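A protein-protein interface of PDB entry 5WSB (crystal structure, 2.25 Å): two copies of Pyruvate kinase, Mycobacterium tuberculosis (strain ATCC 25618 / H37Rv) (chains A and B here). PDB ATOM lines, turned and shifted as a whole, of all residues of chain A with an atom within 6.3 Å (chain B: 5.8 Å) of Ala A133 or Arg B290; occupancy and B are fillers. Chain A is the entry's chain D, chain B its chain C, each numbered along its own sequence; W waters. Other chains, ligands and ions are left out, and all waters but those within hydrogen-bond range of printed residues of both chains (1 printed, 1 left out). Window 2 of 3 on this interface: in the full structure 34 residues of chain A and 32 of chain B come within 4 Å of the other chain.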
ATOM      1  N   VAL A 125      18.461 -30.014 -35.923  1.00  0.00           N
ATOM      2  CA  VAL A 125      19.785 -30.458 -36.368  1.00  0.00           C
ATOM      3  C   VAL A 125      20.825 -29.842 -35.469  1.00  0.00           C
ATOM      4  O   VAL A 125      20.964 -28.621 -35.468  1.00  0.00           O
ATOM      5  CB  VAL A 125      20.094 -29.989 -37.804  1.00  0.00           C
ATOM      6  CG1 VAL A 125      21.487 -30.466 -38.223  1.00  0.00           C
ATOM      7  CG2 VAL A 125      19.051 -30.520 -38.776  1.00  0.00           C
ATOM      8  N   LEU A 126      21.551 -30.664 -34.702  1.00  0.00           N
ATOM      9  CA  LEU A 126      22.637 -30.145 -33.854  1.00  0.00           C
ATOM     10  C   LEU A 126      23.987 -30.468 -34.484  1.00  0.00           C
ATOM     11  O   LEU A 126      24.215 -31.582 -34.946  1.00  0.00           O
ATOM     12  CB  LEU A 126      22.612 -30.741 -32.451  1.00  0.00           C
ATOM     13  CG  LEU A 126      21.432 -30.539 -31.535  1.00  0.00           C
ATOM     14  CD1 LEU A 126      20.640 -29.278 -31.824  1.00  0.00           C
ATOM     15  CD2 LEU A 126      20.550 -31.750 -31.654  1.00  0.00           C
ATOM     16  N   VAL A 127      24.890 -29.500 -34.467  1.00  0.00           N
ATOM     17  CA  VAL A 127      26.131 -29.610 -35.191  1.00  0.00           C
ATOM     18  C   VAL A 127      27.275 -29.571 -34.199  1.00  0.00           C
ATOM     19  O   VAL A 127      27.238 -28.797 -33.222  1.00  0.00           O
ATOM     20  CB  VAL A 127      26.296 -28.420 -36.147  1.00  0.00           C
ATOM     21  CG1 VAL A 127      27.502 -28.636 -37.044  1.00  0.00           C
ATOM     22  CG2 VAL A 127      25.045 -28.227 -36.978  1.00  0.00           C
ATOM     23  N   ASP A 129      28.324 -31.479 -31.986  1.00  0.00           N
ATOM     24  CA  ASP A 129      27.832 -31.857 -30.656  1.00  0.00           C
ATOM     25  C   ASP A 129      27.049 -30.724 -29.913  1.00  0.00           C
ATOM     26  O   ASP A 129      26.953 -30.724 -28.668  1.00  0.00           O
ATOM     27  CB  ASP A 129      28.979 -32.457 -29.795  1.00  0.00           C
ATOM     28  CG  ASP A 129      29.388 -33.884 -30.261  1.00  0.00           C
ATOM     29  OD1 ASP A 129      28.548 -34.563 -30.917  1.00  0.00           O
ATOM     30  OD2 ASP A 129      30.551 -34.318 -29.996  1.00  0.00           O
ATOM     31  N   GLY A 130      26.487 -29.779 -30.682  1.00  0.00           N
ATOM     32  CA  GLY A 130      25.436 -28.847 -30.157  1.00  0.00           C
ATOM     33  C   GLY A 130      25.777 -27.356 -30.122  1.00  0.00           C
ATOM     34  O   GLY A 130      24.944 -26.534 -29.713  1.00  0.00           O
ATOM     35  N   LYS A 131      26.987 -27.005 -30.577  1.00  0.00           N
ATOM     36  CA  LYS A 131      27.456 -25.615 -30.611  1.00  0.00           C
ATOM     37  C   LYS A 131      26.991 -24.879 -31.879  1.00  0.00           C
ATOM     38  O   LYS A 131      27.465 -23.782 -32.205  1.00  0.00           O
ATOM     39  CB  LYS A 131      28.977 -25.571 -30.494  1.00  0.00           C
ATOM     40  CG  LYS A 131      29.480 -25.704 -29.055  1.00  0.00           C
ATOM     41  CD  LYS A 131      29.400 -27.115 -28.467  1.00  0.00           C
ATOM     42  CE  LYS A 131      30.215 -27.178 -27.159  1.00  0.00           C
ATOM     43  NZ  LYS A 131      29.828 -28.274 -26.230  1.00  0.00           N
ATOM     44  N   VAL A 132      26.104 -25.521 -32.609  1.00  0.00           N
ATOM     45  CA  VAL A 132      25.256 -24.839 -33.551  1.00  0.00           C
ATOM     46  C   VAL A 132      24.009 -25.684 -33.625  1.00  0.00           C
ATOM     47  O   VAL A 132      24.099 -26.903 -33.719  1.00  0.00           O
ATOM     48  CB  VAL A 132      25.922 -24.691 -34.919  1.00  0.00           C
ATOM     49  CG1 VAL A 132      24.906 -24.363 -35.993  1.00  0.00           C
ATOM     50  CG2 VAL A 132      26.925 -23.571 -34.852  1.00  0.00           C
ATOM     51  N   ALA A 133      22.845 -25.045 -33.528  1.00  0.00           N
ATOM     52  CA  ALA A 133      21.564 -25.773 -33.638  1.00  0.00           C
ATOM     53  C   ALA A 133      20.681 -25.145 -34.700  1.00  0.00           C
ATOM     54  O   ALA A 133      20.556 -23.911 -34.782  1.00  0.00           O
ATOM     55  CB  ALA A 133      20.844 -25.797 -32.301  1.00  0.00           C
ATOM     56  N   LEU A 134      20.078 -25.991 -35.524  1.00  0.00           N
ATOM     57  CA  LEU A 134      19.218 -25.518 -36.561  1.00  0.00           C
ATOM     58  C   LEU A 134      17.880 -26.187 -36.391  1.00  0.00           C
ATOM     59  O   LEU A 134      17.796 -27.215 -35.746  1.00  0.00           O
ATOM     60  CB  LEU A 134      19.790 -25.850 -37.936  1.00  0.00           C
ATOM     61  CG  LEU A 134      21.291 -25.715 -38.222  1.00  0.00           C
ATOM     62  CD1 LEU A 134      21.546 -26.218 -39.632  1.00  0.00           C
ATOM     63  CD2 LEU A 134      21.806 -24.298 -38.110  1.00  0.00           C
ATOM     64  N   VAL A 135      16.835 -25.579 -36.938  1.00  0.00           N
ATOM     65  CA  VAL A 135      15.568 -26.262 -37.082  1.00  0.00           C
ATOM     66  C   VAL A 135      15.202 -26.306 -38.571  1.00  0.00           C
ATOM     67  O   VAL A 135      15.385 -25.339 -39.304  1.00  0.00           O
ATOM     68  CB  VAL A 135      14.426 -25.613 -36.228  1.00  0.00           C
ATOM     69  CG1 VAL A 135      13.152 -26.425 -36.348  1.00  0.00           C
ATOM     70  CG2 VAL A 135      14.827 -25.538 -34.756  1.00  0.00           C
ATOM     71  N   THR A 147      16.771 -22.983 -40.307  1.00  0.00           N
ATOM     72  CA  THR A 147      17.022 -21.748 -39.649  1.00  0.00           C
ATOM     73  C   THR A 147      17.967 -21.985 -38.508  1.00  0.00           C
ATOM     74  O   THR A 147      17.735 -22.854 -37.673  1.00  0.00           O
ATOM     75  CB  THR A 147      15.708 -21.174 -39.105  1.00  0.00           C
ATOM     76  OG1 THR A 147      14.775 -21.019 -40.182  1.00  0.00           O
ATOM     77  CG2 THR A 147      15.941 -19.841 -38.464  1.00  0.00           C
ATOM     78  N   VAL A 148      19.026 -21.191 -38.447  1.00  0.00           N
ATOM     79  CA  VAL A 148      19.927 -21.266 -37.326  1.00  0.00           C
ATOM     80  C   VAL A 148      19.176 -20.719 -36.129  1.00  0.00           C
ATOM     81  O   VAL A 148      18.764 -19.568 -36.133  1.00  0.00           O
ATOM     82  CB  VAL A 148      21.234 -20.462 -37.562  1.00  0.00           C
ATOM     83  CG1 VAL A 148      22.211 -20.663 -36.395  1.00  0.00           C
ATOM     84  CG2 VAL A 148      21.904 -20.866 -38.882  1.00  0.00           C
ATOM     85  N   VAL A 149      18.967 -21.562 -35.132  1.00  0.00           N
ATOM     86  CA  VAL A 149      18.325 -21.174 -33.913  1.00  0.00           C
ATOM     87  C   VAL A 149      19.356 -20.907 -32.803  1.00  0.00           C
ATOM     88  O   VAL A 149      19.100 -20.125 -31.878  1.00  0.00           O
ATOM     89  CB  VAL A 149      17.343 -22.281 -33.485  1.00  0.00           C
ATOM     90  CG1 VAL A 149      16.883 -22.106 -32.035  1.00  0.00           C
ATOM     91  CG2 VAL A 149      16.166 -22.321 -34.443  1.00  0.00           C
ATOM     92  N   GLU A 150      20.511 -21.568 -32.882  1.00  0.00           N
ATOM     93  CA  GLU A 150      21.625 -21.254 -31.989  1.00  0.00           C
ATOM     94  C   GLU A 150      22.893 -21.160 -32.819  1.00  0.00           C
ATOM     95  O   GLU A 150      23.276 -22.113 -33.495  1.00  0.00           O
ATOM     96  CB  GLU A 150      21.788 -22.320 -30.907  1.00  0.00           C
ATOM     97  CG  GLU A 150      20.528 -22.647 -30.135  1.00  0.00           C
ATOM     98  CD  GLU A 150      20.749 -23.762 -29.133  1.00  0.00           C
ATOM     99  OE1 GLU A 150      19.749 -24.398 -28.750  1.00  0.00           O
ATOM    100  OE2 GLU A 150      21.922 -24.017 -28.739  1.00  0.00           O
ATOM    101  N   GLY A 151      23.548 -20.007 -32.749  1.00  0.00           N
ATOM    102  CA  GLY A 151      24.618 -19.685 -33.675  1.00  0.00           C
ATOM    103  C   GLY A 151      25.986 -20.084 -33.169  1.00  0.00           C
ATOM    104  O   GLY A 151      26.188 -20.312 -31.949  1.00  0.00           O
ATOM    105  N   VAL A 250      23.908 -35.065 -27.223  1.00  0.00           N
ATOM    106  CA  VAL A 250      22.990 -34.518 -28.204  1.00  0.00           C
ATOM    107  C   VAL A 250      21.911 -35.535 -28.573  1.00  0.00           C
ATOM    108  O   VAL A 250      20.814 -35.157 -28.951  1.00  0.00           O
ATOM    109  CB  VAL A 250      23.719 -34.008 -29.475  1.00  0.00           C
ATOM    110  CG1 VAL A 250      24.666 -32.875 -29.122  1.00  0.00           C
ATOM    111  CG2 VAL A 250      24.519 -35.104 -30.127  1.00  0.00           C
ATOM    112  N   LEU A 254      21.098 -33.339 -22.671  1.00  0.00           N
ATOM    113  CA  LEU A 254      22.340 -33.276 -21.963  1.00  0.00           C
ATOM    114  C   LEU A 254      22.197 -33.360 -20.455  1.00  0.00           C
ATOM    115  O   LEU A 254      23.122 -33.800 -19.761  1.00  0.00           O
ATOM    116  CB  LEU A 254      23.152 -32.047 -22.379  1.00  0.00           C
ATOM    117  CG  LEU A 254      22.646 -30.638 -22.112  1.00  0.00           C
ATOM    118  CD1 LEU A 254      22.899 -30.214 -20.668  1.00  0.00           C
ATOM    119  CD2 LEU A 254      23.387 -29.710 -23.054  1.00  0.00           C
ATOM    120  N   SER B 284      31.125 -21.908 -19.613  1.00  0.00           N
ATOM    121  CA  SER B 284      31.171 -21.765 -21.076  1.00  0.00           C
ATOM    122  C   SER B 284      29.913 -21.085 -21.648  1.00  0.00           C
ATOM    123  O   SER B 284      29.928 -20.603 -22.794  1.00  0.00           O
ATOM    124  CB  SER B 284      31.353 -23.134 -21.745  1.00  0.00           C
ATOM    125  OG  SER B 284      30.142 -23.895 -21.695  1.00  0.00           O
ATOM    126  N   MET B 285      28.831 -21.058 -20.865  1.00  0.00           N
ATOM    127  CA  MET B 285      27.586 -20.480 -21.328  1.00  0.00           C
ATOM    128  C   MET B 285      27.649 -18.965 -21.328  1.00  0.00           C
ATOM    129  O   MET B 285      26.750 -18.293 -21.836  1.00  0.00           O
ATOM    130  CB  MET B 285      26.410 -20.973 -20.499  1.00  0.00           C
ATOM    131  CG  MET B 285      26.083 -22.422 -20.781  1.00  0.00           C
ATOM    132  SD  MET B 285      24.427 -22.831 -20.222  1.00  0.00           S
ATOM    133  CE  MET B 285      23.451 -21.926 -21.447  1.00  0.00           C
ATOM    134  N   ASN B 288      28.375 -19.436 -25.056  1.00  0.00           N
ATOM    135  CA  ASN B 288      27.754 -20.531 -25.811  1.00  0.00           C
ATOM    136  C   ASN B 288      26.364 -20.848 -25.277  1.00  0.00           C
ATOM    137  O   ASN B 288      26.090 -20.663 -24.088  1.00  0.00           O
ATOM    138  CB  ASN B 288      28.600 -21.810 -25.675  1.00  0.00           C
ATOM    139  CG  ASN B 288      29.943 -21.740 -26.417  1.00  0.00           C
ATOM    140  OD1 ASN B 288      30.083 -22.288 -27.539  1.00  0.00           O
ATOM    141  ND2 ASN B 288      30.967 -21.183 -25.757  1.00  0.00           N
ATOM    142  N   SER B 289      25.510 -21.371 -26.151  1.00  0.00           N
ATOM    143  CA  SER B 289      24.095 -21.608 -25.830  1.00  0.00           C
ATOM    144  C   SER B 289      23.883 -22.896 -25.041  1.00  0.00           C
ATOM    145  O   SER B 289      22.831 -23.096 -24.443  1.00  0.00           O
ATOM    146  CB  SER B 289      23.315 -21.699 -27.131  1.00  0.00           C
ATOM    147  OG  SER B 289      23.984 -22.610 -28.004  1.00  0.00           O
ATOM    148  N   ARG B 290      24.879 -23.781 -25.086  1.00  0.00           N
ATOM    149  CA  ARG B 290      24.843 -25.044 -24.376  1.00  0.00           C
ATOM    150  C   ARG B 290      26.181 -25.243 -23.671  1.00  0.00           C
ATOM    151  O   ARG B 290      27.231 -24.866 -24.216  1.00  0.00           O
ATOM    152  CB  ARG B 290      24.587 -26.192 -25.347  1.00  0.00           C
ATOM    153  CG  ARG B 290      23.121 -26.353 -25.681  1.00  0.00           C
ATOM    154  CD  ARG B 290      22.892 -26.964 -27.037  1.00  0.00           C
ATOM    155  NE  ARG B 290      21.650 -26.469 -27.638  1.00  0.00           N
ATOM    156  CZ  ARG B 290      20.919 -27.149 -28.515  1.00  0.00           C
ATOM    157  NH1 ARG B 290      21.285 -28.377 -28.895  1.00  0.00           N
ATOM    158  NH2 ARG B 290      19.797 -26.613 -29.011  1.00  0.00           N
ATOM    159  N   PRO B 291      26.144 -25.819 -22.457  1.00  0.00           N
ATOM    160  CA  PRO B 291      27.298 -26.013 -21.640  1.00  0.00           C
ATOM    161  C   PRO B 291      28.120 -27.266 -22.035  1.00  0.00           C
ATOM    162  O   PRO B 291      27.750 -28.025 -22.951  1.00  0.00           O
ATOM    163  CB  PRO B 291      26.699 -26.207 -20.266  1.00  0.00           C
ATOM    164  CG  PRO B 291      25.452 -26.964 -20.535  1.00  0.00           C
ATOM    165  CD  PRO B 291      24.938 -26.368 -21.814  1.00  0.00           C
ATOM    166  N   THR B 292      29.257 -27.454 -21.379  1.00  0.00           N
ATOM    167  CA  THR B 292      30.067 -28.658 -21.641  1.00  0.00           C
ATOM    168  C   THR B 292      29.492 -29.825 -20.840  1.00  0.00           C
ATOM    169  O   THR B 292      28.564 -29.658 -20.030  1.00  0.00           O
ATOM    170  CB  THR B 292      31.540 -28.428 -21.275  1.00  0.00           C
ATOM    171  OG1 THR B 292      31.652 -28.193 -19.866  1.00  0.00           O
ATOM    172  CG2 THR B 292      32.080 -27.217 -22.052  1.00  0.00           C
ATOM    173  N   GLU B 295      30.507 -29.419 -17.314  1.00  0.00           N
ATOM    174  CA  GLU B 295      29.678 -28.441 -16.618  1.00  0.00           C
ATOM    175  C   GLU B 295      28.363 -29.043 -16.166  1.00  0.00           C
ATOM    176  O   GLU B 295      27.925 -28.830 -15.024  1.00  0.00           O
ATOM    177  CB  GLU B 295      29.471 -27.245 -17.521  1.00  0.00           C
ATOM    178  CG  GLU B 295      30.643 -26.294 -17.473  1.00  0.00           C
ATOM    179  CD  GLU B 295      30.758 -25.368 -18.669  1.00  0.00           C
ATOM    180  OE1 GLU B 295      29.888 -25.416 -19.609  1.00  0.00           O
ATOM    181  OE2 GLU B 295      31.745 -24.583 -18.666  1.00  0.00           O
HETATM  182  O   HOH W   1      26.506 -24.142 -27.808  1.00  0.00           O
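Of the printed residues of chain B, Gly A130 touches Arg B290. Printed residues of chain B within 4 Å of Lys A131: Asn B288 and Pro B291. Ala A133 touches just one residue of chain B: Arg B290 (3.5 Å). Gly A151 touches none of the printed residues of chain B. Printed residues of chain A within 4 Å of Asn B288: Lys A131. The nearest residue of chain A that does not touch Arg B290 is Leu A254 (4.3 Å). The nearest printed residue of chain A that does not touch Pro B291 is Asp A129 (6.4 Å).
The side-chain carboxylate (OE2) of Glu A150 sits at hydrogen-bond distance from the side-chain hydroxyl (OG) of Ser B289. The guanidinium group (NE) of Arg B290 is in salt-bridge range of the side-chain carboxylate (OE2) of Glu A150.
Water W1 lies within hydrogen-bond range of the side-chain hydroxyl of Ser B289 (3.0 Å), the backbone NH of Arg B290 (3.2 Å) and the backbone carbonyl oxygen of Gly A130 (3.4 Å).
Of the 17 printed residues of chain A, 6 touch a printed residue of chain B. Hydrophobic or aromatic side chains of chain A that line the printed part of chain B: Leu A126, Ala A133 and Leu A254. Among the printed residues, Asp or Glu carboxylates within 4 Å of a Lys or Arg side-chain nitrogen of the other chain: Glu A150 with Arg B290 (2.2 Å).
O of Ser B284 is in hydrogen-bond range of ND2 of Asn B288. O of Ala A133 is in hydrogen-bond range of N of Val A149 (2.9 Å). N of Ala A133 lies within hydrogen-bond range of O of Glu A150 (3.0 Å).
No position is printed for both chains. Of the 8 pairs that touch across the chains among the printed residues, none has its exchanged pair printed and touching as well.
Among the printed residues, merely in contact across the chains: Leu A126 with Arg B290 (3.1 Å), Gly A130 with Arg B290 (3.4 Å), Ala A133 with Arg B290 (3.5 Å), Lys A131 with Asn B288 (3.8 Å), Leu A254 with Pro B291 (3.9 Å) and Lys A131 with Pro B291 (3.9 Å).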
